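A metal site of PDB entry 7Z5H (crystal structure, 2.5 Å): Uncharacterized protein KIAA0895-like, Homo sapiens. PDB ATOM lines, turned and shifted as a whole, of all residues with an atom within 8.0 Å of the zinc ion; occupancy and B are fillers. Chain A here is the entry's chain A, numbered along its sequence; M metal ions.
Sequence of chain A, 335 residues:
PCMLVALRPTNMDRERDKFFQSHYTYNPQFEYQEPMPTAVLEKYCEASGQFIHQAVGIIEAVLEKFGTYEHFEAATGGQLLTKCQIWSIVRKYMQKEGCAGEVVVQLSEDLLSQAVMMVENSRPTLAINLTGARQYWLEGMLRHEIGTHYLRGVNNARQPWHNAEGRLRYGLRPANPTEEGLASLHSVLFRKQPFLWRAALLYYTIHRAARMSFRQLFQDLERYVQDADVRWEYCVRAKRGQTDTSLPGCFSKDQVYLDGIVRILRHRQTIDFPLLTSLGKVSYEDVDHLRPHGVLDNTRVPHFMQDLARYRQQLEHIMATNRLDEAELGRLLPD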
ATOM      1  N   SER A 113     -21.922  -7.567  20.592  1.00  0.00           N
ATOM      2  CA  SER A 113     -23.105  -6.749  20.876  1.00  0.00           C
ATOM      3  C   SER A 113     -23.248  -5.617  19.852  1.00  0.00           C
ATOM      4  O   SER A 113     -22.428  -5.490  18.953  1.00  0.00           O
ATOM      5  CB  SER A 113     -23.032  -6.167  22.296  1.00  0.00           C
ATOM      6  OG  SER A 113     -21.891  -5.350  22.453  1.00  0.00           O
ATOM      7  N   ALA A 115     -23.022  -2.366  20.472  1.00  0.00           N
ATOM      8  CA  ALA A 115     -21.955  -1.409  20.751  1.00  0.00           C
ATOM      9  C   ALA A 115     -21.299  -1.676  22.096  1.00  0.00           C
ATOM     10  O   ALA A 115     -21.923  -2.224  22.992  1.00  0.00           O
ATOM     11  CB  ALA A 115     -22.515   0.010  20.676  1.00  0.00           C
ATOM     12  N   VAL A 116     -20.039  -1.265  22.228  1.00  0.00           N
ATOM     13  CA  VAL A 116     -19.288  -1.309  23.495  1.00  0.00           C
ATOM     14  C   VAL A 116     -18.564   0.014  23.740  1.00  0.00           C
ATOM     15  O   VAL A 116     -17.845   0.514  22.894  1.00  0.00           O
ATOM     16  CB  VAL A 116     -18.294  -2.490  23.528  1.00  0.00           C
ATOM     17  CG1 VAL A 116     -17.272  -2.392  22.403  1.00  0.00           C
ATOM     18  CG2 VAL A 116     -17.602  -2.573  24.890  1.00  0.00           C
ATOM     19  N   MET A 117     -18.800   0.595  24.915  1.00  0.00           N
ATOM     20  CA  MET A 117     -18.110   1.802  25.366  1.00  0.00           C
ATOM     21  C   MET A 117     -16.809   1.344  26.025  1.00  0.00           C
ATOM     22  O   MET A 117     -16.840   0.449  26.852  1.00  0.00           O
ATOM     23  CB  MET A 117     -19.001   2.576  26.340  1.00  0.00           C
ATOM     24  CG  MET A 117     -18.474   3.947  26.676  1.00  0.00           C
ATOM     25  SD  MET A 117     -18.741   5.073  25.292  1.00  0.00           S
ATOM     26  CE  MET A 117     -17.797   6.492  25.837  1.00  0.00           C
ATOM     27  N   MET A 141     -29.351   2.614  21.416  1.00  0.00           N
ATOM     28  CA  MET A 141     -27.973   2.231  21.755  1.00  0.00           C
ATOM     29  C   MET A 141     -27.208   3.420  22.333  1.00  0.00           C
ATOM     30  O   MET A 141     -26.487   3.292  23.325  1.00  0.00           O
ATOM     31  CB  MET A 141     -27.255   1.691  20.516  1.00  0.00           C
ATOM     32  CG  MET A 141     -25.772   1.328  20.750  1.00  0.00           C
ATOM     33  SD  MET A 141     -24.628   2.717  20.786  1.00  0.00           S
ATOM     34  CE  MET A 141     -24.731   3.274  19.059  1.00  0.00           C
ATOM     35  N   HIS A 144     -28.249   4.227  25.756  1.00  0.00           N
ATOM     36  CA  HIS A 144     -27.657   3.197  26.614  1.00  0.00           C
ATOM     37  C   HIS A 144     -26.186   3.536  26.886  1.00  0.00           C
ATOM     38  O   HIS A 144     -25.799   3.768  28.037  1.00  0.00           O
ATOM     39  CB  HIS A 144     -27.789   1.829  25.920  1.00  0.00           C
ATOM     40  CG  HIS A 144     -27.221   0.685  26.694  1.00  0.00           C
ATOM     41  ND1 HIS A 144     -27.993  -0.370  27.127  1.00  0.00           N
ATOM     42  CD2 HIS A 144     -25.963   0.417  27.113  1.00  0.00           C
ATOM     43  CE1 HIS A 144     -27.233  -1.243  27.779  1.00  0.00           C
ATOM     44  NE2 HIS A 144     -25.992  -0.780  27.784  1.00  0.00           N
ATOM     45  N   GLU A 145     -25.380   3.582  25.819  1.00  0.00           N
ATOM     46  CA  GLU A 145     -23.937   3.686  25.932  1.00  0.00           C
ATOM     47  C   GLU A 145     -23.414   5.077  26.318  1.00  0.00           C
ATOM     48  O   GLU A 145     -22.444   5.187  27.055  1.00  0.00           O
ATOM     49  CB  GLU A 145     -23.284   3.228  24.617  1.00  0.00           C
ATOM     50  CG  GLU A 145     -23.536   1.772  24.244  1.00  0.00           C
ATOM     51  CD  GLU A 145     -22.901   0.782  25.229  1.00  0.00           C
ATOM     52  OE1 GLU A 145     -21.947   1.155  25.937  1.00  0.00           O
ATOM     53  OE2 GLU A 145     -23.364  -0.385  25.290  1.00  0.00           O
ATOM     54  N   THR A 148     -26.299   6.823  29.422  1.00  0.00           N
ATOM     55  CA  THR A 148     -26.193   6.136  30.720  1.00  0.00           C
ATOM     56  C   THR A 148     -24.731   5.859  31.099  1.00  0.00           C
ATOM     57  O   THR A 148     -24.183   6.532  31.972  1.00  0.00           O
ATOM     58  CB  THR A 148     -27.048   4.851  30.738  1.00  0.00           C
ATOM     59  OG1 THR A 148     -28.319   5.106  30.112  1.00  0.00           O
ATOM     60  CG2 THR A 148     -27.283   4.373  32.154  1.00  0.00           C
ATOM     61  N   HIS A 149     -24.077   4.894  30.426  1.00  0.00           N
ATOM     62  CA  HIS A 149     -22.722   4.468  30.802  1.00  0.00           C
ATOM     63  C   HIS A 149     -21.721   5.615  30.838  1.00  0.00           C
ATOM     64  O   HIS A 149     -20.997   5.755  31.828  1.00  0.00           O
ATOM     65  CB  HIS A 149     -22.202   3.343  29.889  1.00  0.00           C
ATOM     66  CG  HIS A 149     -22.955   2.061  30.027  1.00  0.00           C
ATOM     67  ND1 HIS A 149     -23.460   1.616  31.226  1.00  0.00           N
ATOM     68  CD2 HIS A 149     -23.274   1.119  29.114  1.00  0.00           C
ATOM     69  CE1 HIS A 149     -24.089   0.467  31.036  1.00  0.00           C
ATOM     70  NE2 HIS A 149     -23.981   0.140  29.755  1.00  0.00           N
ATOM     71  N   ASN A 176     -23.520  -2.656  39.176  1.00  0.00           N
ATOM     72  CA  ASN A 176     -24.483  -3.576  38.604  1.00  0.00           C
ATOM     73  C   ASN A 176     -25.261  -4.263  39.728  1.00  0.00           C
ATOM     74  O   ASN A 176     -24.716  -4.494  40.794  1.00  0.00           O
ATOM     75  CB  ASN A 176     -23.787  -4.600  37.722  1.00  0.00           C
ATOM     76  CG  ASN A 176     -23.606  -4.109  36.299  1.00  0.00           C
ATOM     77  OD1 ASN A 176     -24.420  -3.352  35.793  1.00  0.00           O
ATOM     78  ND2 ASN A 176     -22.536  -4.558  35.643  1.00  0.00           N
ATOM     79  N   GLU A 179     -26.571  -0.379  36.930  1.00  0.00           N
ATOM     80  CA  GLU A 179     -25.952   0.239  35.758  1.00  0.00           C
ATOM     81  C   GLU A 179     -26.597  -0.215  34.450  1.00  0.00           C
ATOM     82  O   GLU A 179     -27.114   0.599  33.671  1.00  0.00           O
ATOM     83  CB  GLU A 179     -24.440  -0.049  35.758  1.00  0.00           C
ATOM     84  CG  GLU A 179     -23.653   0.665  34.666  1.00  0.00           C
ATOM     85  CD  GLU A 179     -23.587   2.170  34.841  1.00  0.00           C
ATOM     86  OE1 GLU A 179     -23.817   2.656  35.971  1.00  0.00           O
ATOM     87  OE2 GLU A 179     -23.305   2.859  33.839  1.00  0.00           O
ATOM     88  N   GLU A 180     -26.550  -1.525  34.189  1.00  0.00           N
ATOM     89  CA  GLU A 180     -27.039  -2.103  32.950  1.00  0.00           C
ATOM     90  C   GLU A 180     -28.557  -2.189  32.904  1.00  0.00           C
ATOM     91  O   GLU A 180     -29.133  -2.247  31.825  1.00  0.00           O
ATOM     92  CB  GLU A 180     -26.416  -3.475  32.732  1.00  0.00           C
ATOM     93  CG  GLU A 180     -24.906  -3.444  32.528  1.00  0.00           C
ATOM     94  CD  GLU A 180     -24.467  -2.886  31.197  1.00  0.00           C
ATOM     95  OE1 GLU A 180     -25.268  -2.217  30.492  1.00  0.00           O
ATOM     96  OE2 GLU A 180     -23.288  -3.115  30.835  1.00  0.00           O
ATOM     97  N   GLY A 181     -29.203  -2.196  34.077  1.00  0.00           N
ATOM     98  CA  GLY A 181     -30.648  -2.091  34.202  1.00  0.00           C
ATOM     99  C   GLY A 181     -31.150  -0.752  33.703  1.00  0.00           C
ATOM    100  O   GLY A 181     -32.081  -0.693  32.898  1.00  0.00           O
ATOM    101  N   ALA A 183     -29.413   1.355  31.808  1.00  0.00           N
ATOM    102  CA  ALA A 183     -28.990   1.470  30.416  1.00  0.00           C
ATOM    103  C   ALA A 183     -29.964   0.763  29.458  1.00  0.00           C
ATOM    104  O   ALA A 183     -30.247   1.261  28.370  1.00  0.00           O
ATOM    105  CB  ALA A 183     -27.583   0.921  30.250  1.00  0.00           C
ATOM    106  N   SER A 184     -30.467  -0.410  29.879  1.00  0.00           N
ATOM    107  CA  SER A 184     -31.408  -1.213  29.094  1.00  0.00           C
ATOM    108  C   SER A 184     -32.792  -0.575  29.000  1.00  0.00           C
ATOM    109  O   SER A 184     -33.415  -0.617  27.945  1.00  0.00           O
ATOM    110  CB  SER A 184     -31.541  -2.627  29.672  1.00  0.00           C
ATOM    111  OG  SER A 184     -30.349  -3.354  29.464  1.00  0.00           O
ATOM    112  N   SER A 187     -32.518   2.297  26.547  1.00  0.00           N
ATOM    113  CA  SER A 187     -32.390   1.895  25.139  1.00  0.00           C
ATOM    114  C   SER A 187     -33.755   1.868  24.454  1.00  0.00           C
ATOM    115  O   SER A 187     -33.898   2.244  23.292  1.00  0.00           O
ATOM    116  CB  SER A 187     -31.700   0.529  24.951  1.00  0.00           C
ATOM    117  OG  SER A 187     -30.547   0.285  25.720  1.00  0.00           O
ATOM    118  N   ARG A 237     -21.940 -15.624  23.847  1.00  0.00           N
ATOM    119  CA  ARG A 237     -22.103 -14.715  24.968  1.00  0.00           C
ATOM    120  C   ARG A 237     -22.419 -15.447  26.274  1.00  0.00           C
ATOM    121  O   ARG A 237     -21.880 -15.086  27.329  1.00  0.00           O
ATOM    122  CB  ARG A 237     -23.193 -13.686  24.678  1.00  0.00           C
ATOM    123  CG  ARG A 237     -22.765 -12.575  23.740  1.00  0.00           C
ATOM    124  CD  ARG A 237     -23.870 -11.558  23.654  1.00  0.00           C
ATOM    125  NE  ARG A 237     -24.049 -10.705  24.838  1.00  0.00           N
ATOM    126  CZ  ARG A 237     -23.356  -9.601  25.100  1.00  0.00           C
ATOM    127  NH1 ARG A 237     -22.352  -9.228  24.308  1.00  0.00           N
ATOM    128  NH2 ARG A 237     -23.608  -8.901  26.201  1.00  0.00           N
ATOM    129  N   VAL A 256     -27.591  -9.682  34.035  1.00  0.00           N
ATOM    130  CA  VAL A 256     -27.634  -8.400  34.727  1.00  0.00           C
ATOM    131  C   VAL A 256     -28.693  -7.451  34.160  1.00  0.00           C
ATOM    132  O   VAL A 256     -29.314  -6.696  34.924  1.00  0.00           O
ATOM    133  CB  VAL A 256     -26.248  -7.739  34.702  1.00  0.00           C
ATOM    134  CG1 VAL A 256     -25.865  -7.307  33.282  1.00  0.00           C
ATOM    135  CG2 VAL A 256     -26.202  -6.617  35.661  1.00  0.00           C
ATOM    136  N   TYR A 257     -28.903  -7.500  32.834  1.00  0.00           N
ATOM    137  CA  TYR A 257     -29.808  -6.584  32.142  1.00  0.00           C
ATOM    138  C   TYR A 257     -31.242  -6.713  32.661  1.00  0.00           C
ATOM    139  O   TYR A 257     -31.817  -5.735  33.151  1.00  0.00           O
ATOM    140  CB  TYR A 257     -29.750  -6.812  30.636  1.00  0.00           C
ATOM    141  CG  TYR A 257     -28.378  -6.577  30.042  1.00  0.00           C
ATOM    142  CD1 TYR A 257     -27.879  -5.302  29.913  1.00  0.00           C
ATOM    143  CD2 TYR A 257     -27.609  -7.635  29.600  1.00  0.00           C
ATOM    144  CE1 TYR A 257     -26.626  -5.075  29.367  1.00  0.00           C
ATOM    145  CE2 TYR A 257     -26.338  -7.419  29.052  1.00  0.00           C
ATOM    146  CZ  TYR A 257     -25.869  -6.136  28.931  1.00  0.00           C
ATOM    147  OH  TYR A 257     -24.639  -5.905  28.370  1.00  0.00           O
HETATM  148 ZN    ZN M   1     -24.215  -1.807  28.562  1.00  0.00          ZN
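The zinc ion is bound by a ring nitrogen (NE2) of His 144 (2.2 Å), the side-chain carboxylate of Glu 180 (2.2 Å) and a ring nitrogen (NE2) of His 149 (2.3 Å).
The zinc ion has three donor atoms within binding distance.
Slightly farther from the zinc ion lies the side-chain carboxylate (OE2) of Glu 180 (2.8 Å).
A ring nitrogen (ND1) of His 144 lies within hydrogen-bond range of the side-chain hydroxyl of Ser 187 (3.0 Å).
The side-chain carboxylate of Glu 179 lies within hydrogen-bond range of a ring nitrogen (ND1) of His 149 (2.9 Å).
OE1 of Glu 145 sits close to N of Met 117 (3.4 Å).
The backbone NH (N) of Glu 180 lies within hydrogen-bond range of the side-chain amide oxygen (OD1) of Asn 176, 3.2 Å away.
ND1 of His 144 sits at hydrogen-bond distance from O of Ala 183 (3.0 Å).
O of Glu 180 is in hydrogen-bond range of OG of Ser 184, at 2.9 Å.
Residues that only touch the zinc ion: Glu 145 (3.7 Å).
Of the 19 residues printed, 4 come within 4 Å of the zinc ion.
Along chain A the residues within 4 Å of the zinc ion span positions 144 to 180.
The nearest printed residue that does not touch the zinc ion is Tyr 257 (4.1 Å).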
